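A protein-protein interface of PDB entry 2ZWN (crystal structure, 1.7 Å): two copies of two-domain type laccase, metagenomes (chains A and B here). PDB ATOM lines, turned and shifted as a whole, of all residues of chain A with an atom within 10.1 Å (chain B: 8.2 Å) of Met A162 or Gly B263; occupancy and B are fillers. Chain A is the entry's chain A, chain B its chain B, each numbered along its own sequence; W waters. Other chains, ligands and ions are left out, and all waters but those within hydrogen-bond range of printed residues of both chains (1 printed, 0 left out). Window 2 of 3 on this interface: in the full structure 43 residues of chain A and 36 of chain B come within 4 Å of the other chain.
The side-chain amide oxygen of Asn A110 sits close to a ring nitrogen (ND1) of His B265 (3.4 Å).
The backbone NH (N) of Gly A159 is in hydrogen-bond range of the side-chain amide oxygen (OD1) of Asn A163 (3.4 Å).
The side-chain amide oxygen of Asn A163 lies within hydrogen-bond range of the side-chain hydroxyl of Thr A160.
The side-chain hydroxyl (OG1) of Thr B260 is in hydrogen-bond range of the backbone carbonyl oxygen (O) of Thr B257 (2.6 Å).
The side-chain hydroxyl (OG1) of Thr A160 sits close to the backbone NH (N) of Met A162 (3.3 Å).
The side-chain amide nitrogen (ND2) of Asn A110 sits at hydrogen-bond distance from the backbone carbonyl oxygen (O) of Gly A158 (3.4 Å).
O of Gly A159 lies close to ND2 of Asn A110 (3.2 Å).
His B265 touches Asn A108.
Thr B260 touches Asn A110.
Thr B257 touches Gly A159 (CG2 to O, 3.6 Å).
Thr A160 touches Thr B257.
Thr A160 touches Gly B263 (CG2 to O, 3.5 Å).
Pro A161 touches Ala B165 (CB to O, 3.4 Å).
Pro A161 touches Phe B168 (CG to CZ, 3.8 Å).
Pro A161 touches Thr B257.
SD of Met A162 touches CG1 of Val B164, at 3.95 Å.
Gly B263 touches Met A162.
Met A162 touches two residues of chain B.
Gly B263 touches just these residues of chain A: Thr A160 and Met A162.
No residue of chain A comes within 4 Å of Ala B261.
Of the printed residues of chain A, Thr B260 touches Asn A110 (3.5 Å) and Pro A161 (3.7 Å).
Printed residues of chain A within 4 Å of Ala B165: Pro A161.
Of the printed residues of chain B, Pro A161 touches Ala B165, Phe B168, Thr B257 and Thr B260.
Of the printed residues of chain B, Thr A160 touches Thr B257 and Gly B263.
Of the 16 printed residues of chain A, 6 touch a printed residue of chain B.
Hydrophobic or aromatic side chains of chain A that line the printed part of chain B: Pro A161 and Met A162.
Of the 15 printed residues of chain B, 7 touch a printed residue of chain A.
Hydrophobic or aromatic side chains of chain B within 4 Å of the printed part of chain A: Val B164, Phe B168 and His B265.
Among the printed residues, 12 pairs touch across the chains.
Among the printed residues, no Asp or Glu carboxylate lies within 4 Å of a Lys or Arg side-chain nitrogen of the other chain.
2 positions are printed for both chains.
Water W1 lies within hydrogen-bond range of the backbone carbonyl oxygen (O) of Gly B263 (2.9 Å) and the side-chain amide nitrogen (ND2) of Asn A110 (3.0 Å).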
ATOM      1  N   ASN A 108     -15.851   5.348 -22.910  1.00  0.00           N
ATOM      2  CA  ASN A 108     -15.449   4.376 -21.885  1.00  0.00           C
ATOM      3  C   ASN A 108     -15.132   5.073 -20.555  1.00  0.00           C
ATOM      4  O   ASN A 108     -14.101   4.806 -19.924  1.00  0.00           O
ATOM      5  CB  ASN A 108     -14.235   3.580 -22.377  1.00  0.00           C
ATOM      6  CG  ASN A 108     -14.530   2.766 -23.637  1.00  0.00           C
ATOM      7  OD1 ASN A 108     -15.672   2.376 -23.888  1.00  0.00           O
ATOM      8  ND2 ASN A 108     -13.497   2.507 -24.430  1.00  0.00           N
ATOM      9  N   ASN A 110     -15.991   5.158 -17.396  1.00  0.00           N
ATOM     10  CA  ASN A 110     -15.646   4.447 -16.166  1.00  0.00           C
ATOM     11  C   ASN A 110     -14.146   4.172 -16.060  1.00  0.00           C
ATOM     12  O   ASN A 110     -13.568   4.304 -14.981  1.00  0.00           O
ATOM     13  CB  ASN A 110     -16.468   3.157 -16.003  1.00  0.00           C
ATOM     14  CG  ASN A 110     -16.256   2.175 -17.130  1.00  0.00           C
ATOM     15  OD1 ASN A 110     -16.500   2.491 -18.293  1.00  0.00           O
ATOM     16  ND2 ASN A 110     -15.808   0.972 -16.792  1.00  0.00           N
ATOM     17  N   GLU A 111     -13.517   3.822 -17.183  1.00  0.00           N
ATOM     18  CA  GLU A 111     -12.075   3.575 -17.216  1.00  0.00           C
ATOM     19  C   GLU A 111     -11.259   4.826 -17.549  1.00  0.00           C
ATOM     20  O   GLU A 111     -10.295   5.149 -16.854  1.00  0.00           O
ATOM     21  CB  GLU A 111     -11.734   2.489 -18.240  1.00  0.00           C
ATOM     22  CG  GLU A 111     -10.270   2.051 -18.171  1.00  0.00           C
ATOM     23  CD  GLU A 111      -9.732   1.462 -19.462  1.00  0.00           C
ATOM     24  OE1 GLU A 111     -10.530   0.996 -20.313  1.00  0.00           O
ATOM     25  OE2 GLU A 111      -8.488   1.459 -19.627  1.00  0.00           O
ATOM     26  N   GLU A 148      -6.779   2.233  -9.358  1.00  0.00           N
ATOM     27  CA  GLU A 148      -6.895   0.801  -9.098  1.00  0.00           C
ATOM     28  C   GLU A 148      -5.595   0.129  -9.525  1.00  0.00           C
ATOM     29  O   GLU A 148      -5.340  -0.022 -10.716  1.00  0.00           O
ATOM     30  CB  GLU A 148      -8.074   0.231  -9.889  1.00  0.00           C
ATOM     31  CG  GLU A 148      -9.419   0.851  -9.512  1.00  0.00           C
ATOM     32  CD  GLU A 148     -10.500   0.653 -10.555  1.00  0.00           C
ATOM     33  OE1 GLU A 148     -10.268  -0.065 -11.548  1.00  0.00           O
ATOM     34  OE2 GLU A 148     -11.599   1.229 -10.386  1.00  0.00           O
ATOM     35  N   ALA A 150      -4.489  -2.841  -9.650  1.00  0.00           N
ATOM     36  CA  ALA A 150      -4.578  -4.092 -10.407  1.00  0.00           C
ATOM     37  C   ALA A 150      -4.580  -3.881 -11.927  1.00  0.00           C
ATOM     38  O   ALA A 150      -4.184  -4.777 -12.669  1.00  0.00           O
ATOM     39  CB  ALA A 150      -5.815  -4.873  -9.983  1.00  0.00           C
ATOM     40  N   VAL A 151      -5.025  -2.710 -12.383  1.00  0.00           N
ATOM     41  CA  VAL A 151      -5.081  -2.398 -13.818  1.00  0.00           C
ATOM     42  C   VAL A 151      -4.093  -1.294 -14.227  1.00  0.00           C
ATOM     43  O   VAL A 151      -4.232  -0.698 -15.292  1.00  0.00           O
ATOM     44  CB  VAL A 151      -6.515  -2.020 -14.255  1.00  0.00           C
ATOM     45  CG1 VAL A 151      -7.471  -3.175 -13.973  1.00  0.00           C
ATOM     46  CG2 VAL A 151      -6.985  -0.735 -13.554  1.00  0.00           C
ATOM     47  N   GLY A 156      -7.725  -0.823 -21.195  1.00  0.00           N
ATOM     48  CA  GLY A 156      -8.888  -1.634 -21.556  1.00  0.00           C
ATOM     49  C   GLY A 156      -9.561  -2.355 -20.398  1.00  0.00           C
ATOM     50  O   GLY A 156     -10.541  -3.077 -20.607  1.00  0.00           O
ATOM     51  N   GLU A 157      -9.040  -2.171 -19.185  1.00  0.00           N
ATOM     52  CA  GLU A 157      -9.640  -2.739 -17.976  1.00  0.00           C
ATOM     53  C   GLU A 157      -9.748  -1.676 -16.888  1.00  0.00           C
ATOM     54  O   GLU A 157      -9.057  -0.662 -16.937  1.00  0.00           O
ATOM     55  CB  GLU A 157      -8.800  -3.908 -17.455  1.00  0.00           C
ATOM     56  CG  GLU A 157      -8.653  -5.060 -18.439  1.00  0.00           C
ATOM     57  CD  GLU A 157      -7.806  -6.206 -17.898  1.00  0.00           C
ATOM     58  OE1 GLU A 157      -7.875  -6.494 -16.681  1.00  0.00           O
ATOM     59  OE2 GLU A 157      -7.073  -6.828 -18.701  1.00  0.00           O
ATOM     60  N   GLY A 158     -10.620  -1.924 -15.909  1.00  0.00           N
ATOM     61  CA  GLY A 158     -10.750  -1.065 -14.732  1.00  0.00           C
ATOM     62  C   GLY A 158     -11.996  -0.200 -14.718  1.00  0.00           C
ATOM     63  O   GLY A 158     -12.733  -0.126 -15.701  1.00  0.00           O
ATOM     64  N   GLY A 159     -12.224   0.445 -13.582  1.00  0.00           N
ATOM     65  CA  GLY A 159     -13.332   1.378 -13.412  1.00  0.00           C
ATOM     66  C   GLY A 159     -14.683   0.718 -13.221  1.00  0.00           C
ATOM     67  O   GLY A 159     -15.706   1.300 -13.561  1.00  0.00           O
ATOM     68  N   THR A 160     -14.695  -0.495 -12.680  1.00  0.00           N
ATOM     69  CA  THR A 160     -15.945  -1.195 -12.405  1.00  0.00           C
ATOM     70  C   THR A 160     -16.125  -1.404 -10.901  1.00  0.00           C
ATOM     71  O   THR A 160     -15.159  -1.300 -10.134  1.00  0.00           O
ATOM     72  CB  THR A 160     -15.995  -2.561 -13.121  1.00  0.00           C
ATOM     73  OG1 THR A 160     -15.171  -3.502 -12.425  1.00  0.00           O
ATOM     74  CG2 THR A 160     -15.523  -2.428 -14.569  1.00  0.00           C
ATOM     75  N   PRO A 161     -17.364  -1.699 -10.468  1.00  0.00           N
ATOM     76  CA  PRO A 161     -17.610  -2.038  -9.062  1.00  0.00           C
ATOM     77  C   PRO A 161     -16.796  -3.231  -8.537  1.00  0.00           C
ATOM     78  O   PRO A 161     -16.609  -3.350  -7.327  1.00  0.00           O
ATOM     79  CB  PRO A 161     -19.113  -2.363  -9.036  1.00  0.00           C
ATOM     80  CG  PRO A 161     -19.681  -1.647 -10.206  1.00  0.00           C
ATOM     81  CD  PRO A 161     -18.613  -1.687 -11.255  1.00  0.00           C
ATOM     82  N   MET A 162     -16.325  -4.095  -9.436  1.00  0.00           N
ATOM     83  CA  MET A 162     -15.539  -5.273  -9.056  1.00  0.00           C
ATOM     84  C   MET A 162     -14.040  -4.989  -8.870  1.00  0.00           C
ATOM     85  O   MET A 162     -13.312  -5.836  -8.356  1.00  0.00           O
ATOM     86  CB  MET A 162     -15.728  -6.387 -10.090  1.00  0.00           C
ATOM     87  CG  MET A 162     -17.084  -7.091 -10.004  1.00  0.00           C
ATOM     88  SD  MET A 162     -18.497  -6.046 -10.433  1.00  0.00           S
ATOM     89  CE  MET A 162     -18.135  -5.639 -12.136  1.00  0.00           C
ATOM     90  N   ASN A 163     -13.580  -3.820  -9.310  1.00  0.00           N
ATOM     91  CA  ASN A 163     -12.207  -3.391  -9.052  1.00  0.00           C
ATOM     92  C   ASN A 163     -12.107  -2.743  -7.677  1.00  0.00           C
ATOM     93  O   ASN A 163     -13.116  -2.324  -7.102  1.00  0.00           O
ATOM     94  CB  ASN A 163     -11.744  -2.381 -10.103  1.00  0.00           C
ATOM     95  CG  ASN A 163     -11.704  -2.959 -11.502  1.00  0.00           C
ATOM     96  OD1 ASN A 163     -12.577  -2.683 -12.324  1.00  0.00           O
ATOM     97  ND2 ASN A 163     -10.682  -3.763 -11.784  1.00  0.00           N
ATOM     98  N   VAL A 164     -10.883  -2.656  -7.157  1.00  0.00           N
ATOM     99  CA  VAL A 164     -10.626  -2.030  -5.866  1.00  0.00           C
ATOM    100  C   VAL A 164      -9.772  -0.787  -6.076  1.00  0.00           C
ATOM    101  O   VAL A 164      -8.655  -0.883  -6.584  1.00  0.00           O
ATOM    102  CB  VAL A 164      -9.874  -2.992  -4.915  1.00  0.00           C
ATOM    103  CG1 VAL A 164      -9.649  -2.337  -3.559  1.00  0.00           C
ATOM    104  CG2 VAL A 164     -10.642  -4.305  -4.761  1.00  0.00           C
ATOM    105  N   ALA A 165     -10.303   0.377  -5.704  1.00  0.00           N
ATOM    106  CA  ALA A 165      -9.525   1.615  -5.719  1.00  0.00           C
ATOM    107  C   ALA A 165      -8.707   1.671  -4.439  1.00  0.00           C
ATOM    108  O   ALA A 165      -9.267   1.779  -3.340  1.00  0.00           O
ATOM    109  CB  ALA A 165     -10.431   2.838  -5.839  1.00  0.00           C
ATOM    110  N   SER B 149     -26.613  -8.175  -8.936  1.00  0.00           N
ATOM    111  CA  SER B 149     -27.024  -9.254  -9.844  1.00  0.00           C
ATOM    112  C   SER B 149     -26.989 -10.647  -9.195  1.00  0.00           C
ATOM    113  O   SER B 149     -27.772 -11.523  -9.574  1.00  0.00           O
ATOM    114  CB  SER B 149     -26.188  -9.236 -11.129  1.00  0.00           C
ATOM    115  OG  SER B 149     -24.826  -9.517 -10.863  1.00  0.00           O
ATOM    116  N   VAL B 164     -22.219  -7.059  -3.907  1.00  0.00           N
ATOM    117  CA  VAL B 164     -21.674  -6.130  -4.882  1.00  0.00           C
ATOM    118  C   VAL B 164     -22.806  -5.534  -5.706  1.00  0.00           C
ATOM    119  O   VAL B 164     -23.520  -6.261  -6.403  1.00  0.00           O
ATOM    120  CB  VAL B 164     -20.682  -6.826  -5.829  1.00  0.00           C
ATOM    121  CG1 VAL B 164     -20.122  -5.830  -6.835  1.00  0.00           C
ATOM    122  CG2 VAL B 164     -19.563  -7.493  -5.026  1.00  0.00           C
ATOM    123  N   ALA B 165     -22.976  -4.216  -5.614  1.00  0.00           N
ATOM    124  CA  ALA B 165     -23.910  -3.515  -6.486  1.00  0.00           C
ATOM    125  C   ALA B 165     -23.237  -3.312  -7.832  1.00  0.00           C
ATOM    126  O   ALA B 165     -22.282  -2.540  -7.942  1.00  0.00           O
ATOM    127  CB  ALA B 165     -24.323  -2.173  -5.884  1.00  0.00           C
ATOM    128  N   ASP B 166     -23.723  -4.019  -8.848  1.00  0.00           N
ATOM    129  CA  ASP B 166     -23.089  -3.998 -10.163  1.00  0.00           C
ATOM    130  C   ASP B 166     -23.988  -3.497 -11.301  1.00  0.00           C
ATOM    131  O   ASP B 166     -23.545  -3.432 -12.442  1.00  0.00           O
ATOM    132  CB  ASP B 166     -22.468  -5.370 -10.494  1.00  0.00           C
ATOM    133  CG  ASP B 166     -23.469  -6.530 -10.445  1.00  0.00           C
ATOM    134  OD1 ASP B 166     -24.589  -6.384  -9.908  1.00  0.00           O
ATOM    135  OD2 ASP B 166     -23.105  -7.623 -10.941  1.00  0.00           O
ATOM    136  N   TYR B 167     -25.234  -3.139 -10.991  1.00  0.00           N
ATOM    137  CA  TYR B 167     -26.112  -2.464 -11.949  1.00  0.00           C
ATOM    138  C   TYR B 167     -26.746  -1.239 -11.284  1.00  0.00           C
ATOM    139  O   TYR B 167     -26.894  -1.189 -10.058  1.00  0.00           O
ATOM    140  CB  TYR B 167     -27.198  -3.407 -12.480  1.00  0.00           C
ATOM    141  CG  TYR B 167     -26.699  -4.512 -13.395  1.00  0.00           C
ATOM    142  CD1 TYR B 167     -26.926  -4.465 -14.772  1.00  0.00           C
ATOM    143  CD2 TYR B 167     -26.015  -5.608 -12.883  1.00  0.00           C
ATOM    144  CE1 TYR B 167     -26.488  -5.484 -15.608  1.00  0.00           C
ATOM    145  CE2 TYR B 167     -25.563  -6.626 -13.712  1.00  0.00           C
ATOM    146  CZ  TYR B 167     -25.802  -6.558 -15.070  1.00  0.00           C
ATOM    147  OH  TYR B 167     -25.353  -7.574 -15.890  1.00  0.00           O
ATOM    148  N   PHE B 168     -27.099  -0.255 -12.106  1.00  0.00           N
ATOM    149  CA  PHE B 168     -27.525   1.061 -11.635  1.00  0.00           C
ATOM    150  C   PHE B 168     -28.617   1.580 -12.555  1.00  0.00           C
ATOM    151  O   PHE B 168     -28.598   1.303 -13.747  1.00  0.00           O
ATOM    152  CB  PHE B 168     -26.321   2.003 -11.619  1.00  0.00           C
ATOM    153  CG  PHE B 168     -25.131   1.421 -10.929  1.00  0.00           C
ATOM    154  CD1 PHE B 168     -24.979   1.548  -9.556  1.00  0.00           C
ATOM    155  CD2 PHE B 168     -24.184   0.699 -11.643  1.00  0.00           C
ATOM    156  CE1 PHE B 168     -23.891   0.981  -8.915  1.00  0.00           C
ATOM    157  CE2 PHE B 168     -23.094   0.131 -11.005  1.00  0.00           C
ATOM    158  CZ  PHE B 168     -22.950   0.272  -9.641  1.00  0.00           C
ATOM    159  N   THR B 257     -18.090   4.519 -11.826  1.00  0.00           N
ATOM    160  CA  THR B 257     -18.456   3.094 -11.803  1.00  0.00           C
ATOM    161  C   THR B 257     -19.943   2.844 -12.059  1.00  0.00           C
ATOM    162  O   THR B 257     -20.340   1.711 -12.348  1.00  0.00           O
ATOM    163  CB  THR B 257     -18.091   2.428 -10.456  1.00  0.00           C
ATOM    164  OG1 THR B 257     -18.688   3.160  -9.376  1.00  0.00           O
ATOM    165  CG2 THR B 257     -16.582   2.375 -10.274  1.00  0.00           C
ATOM    166  N   VAL B 259     -21.814   4.168 -14.476  1.00  0.00           N
ATOM    167  CA  VAL B 259     -22.174   4.117 -15.892  1.00  0.00           C
ATOM    168  C   VAL B 259     -21.673   2.808 -16.503  1.00  0.00           C
ATOM    169  O   VAL B 259     -21.098   2.782 -17.592  1.00  0.00           O
ATOM    170  CB  VAL B 259     -21.703   5.370 -16.678  1.00  0.00           C
ATOM    171  CG1 VAL B 259     -22.485   6.603 -16.208  1.00  0.00           C
ATOM    172  CG2 VAL B 259     -20.221   5.593 -16.530  1.00  0.00           C
ATOM    173  N   THR B 260     -21.910   1.723 -15.766  1.00  0.00           N
ATOM    174  CA  THR B 260     -21.603   0.368 -16.193  1.00  0.00           C
ATOM    175  C   THR B 260     -22.815  -0.520 -15.916  1.00  0.00           C
ATOM    176  O   THR B 260     -23.737  -0.129 -15.192  1.00  0.00           O
ATOM    177  CB  THR B 260     -20.373  -0.216 -15.458  1.00  0.00           C
ATOM    178  OG1 THR B 260     -20.630  -0.300 -14.048  1.00  0.00           O
ATOM    179  CG2 THR B 260     -19.127   0.645 -15.706  1.00  0.00           C
ATOM    180  N   ALA B 261     -22.799  -1.710 -16.506  1.00  0.00           N
ATOM    181  CA  ALA B 261     -23.831  -2.715 -16.288  1.00  0.00           C
ATOM    182  C   ALA B 261     -23.164  -4.077 -16.234  1.00  0.00           C
ATOM    183  O   ALA B 261     -22.734  -4.598 -17.257  1.00  0.00           O
ATOM    184  CB  ALA B 261     -24.857  -2.671 -17.405  1.00  0.00           C
ATOM    185  N   GLY B 262     -23.052  -4.644 -15.040  1.00  0.00           N
ATOM    186  CA  GLY B 262     -22.366  -5.914 -14.866  1.00  0.00           C
ATOM    187  C   GLY B 262     -20.934  -5.899 -15.374  1.00  0.00           C
ATOM    188  O   GLY B 262     -20.476  -6.857 -16.011  1.00  0.00           O
ATOM    189  N   GLY B 263     -20.227  -4.806 -15.099  1.00  0.00           N
ATOM    190  CA  GLY B 263     -18.820  -4.678 -15.465  1.00  0.00           C
ATOM    191  C   GLY B 263     -18.559  -4.129 -16.856  1.00  0.00           C
ATOM    192  O   GLY B 263     -17.408  -3.856 -17.201  1.00  0.00           O
ATOM    193  N   LYS B 264     -19.605  -3.958 -17.662  1.00  0.00           N
ATOM    194  CA  LYS B 264     -19.417  -3.461 -19.026  1.00  0.00           C
ATOM    195  C   LYS B 264     -20.066  -2.096 -19.225  1.00  0.00           C
ATOM    196  O   LYS B 264     -20.977  -1.713 -18.494  1.00  0.00           O
ATOM    197  CB  LYS B 264     -19.878  -4.487 -20.068  1.00  0.00           C
ATOM    198  CG  LYS B 264     -21.343  -4.837 -20.050  1.00  0.00           C
ATOM    199  CD  LYS B 264     -21.591  -6.255 -20.584  1.00  0.00           C
ATOM    200  CE  LYS B 264     -23.072  -6.620 -20.517  1.00  0.00           C
ATOM    201  NZ  LYS B 264     -23.622  -6.523 -19.126  1.00  0.00           N
ATOM    202  N   HIS B 265     -19.556  -1.361 -20.207  1.00  0.00           N
ATOM    203  CA  HIS B 265     -19.958   0.016 -20.460  1.00  0.00           C
ATOM    204  C   HIS B 265     -20.481   0.115 -21.893  1.00  0.00           C
ATOM    205  O   HIS B 265     -19.993  -0.591 -22.772  1.00  0.00           O
ATOM    206  CB  HIS B 265     -18.753   0.944 -20.245  1.00  0.00           C
ATOM    207  CG  HIS B 265     -19.000   2.375 -20.624  1.00  0.00           C
ATOM    208  ND1 HIS B 265     -19.434   3.324 -19.721  1.00  0.00           N
ATOM    209  CD2 HIS B 265     -18.862   3.020 -21.808  1.00  0.00           C
ATOM    210  CE1 HIS B 265     -19.563   4.487 -20.336  1.00  0.00           C
ATOM    211  NE2 HIS B 265     -19.217   4.332 -21.600  1.00  0.00           N
ATOM    212  N   PRO B 266     -21.483   0.981 -22.139  1.00  0.00           N
ATOM    213  CA  PRO B 266     -22.172   1.845 -21.198  1.00  0.00           C
ATOM    214  C   PRO B 266     -23.375   1.163 -20.562  1.00  0.00           C
ATOM    215  O   PRO B 266     -23.859   0.145 -21.049  1.00  0.00           O
ATOM    216  CB  PRO B 266     -22.636   2.998 -22.081  1.00  0.00           C
ATOM    217  CG  PRO B 266     -22.939   2.349 -23.382  1.00  0.00           C
ATOM    218  CD  PRO B 266     -22.029   1.142 -23.498  1.00  0.00           C
HETATM  219  O   HOH W   1     -16.221  -1.549 -18.398  1.00  0.00           O
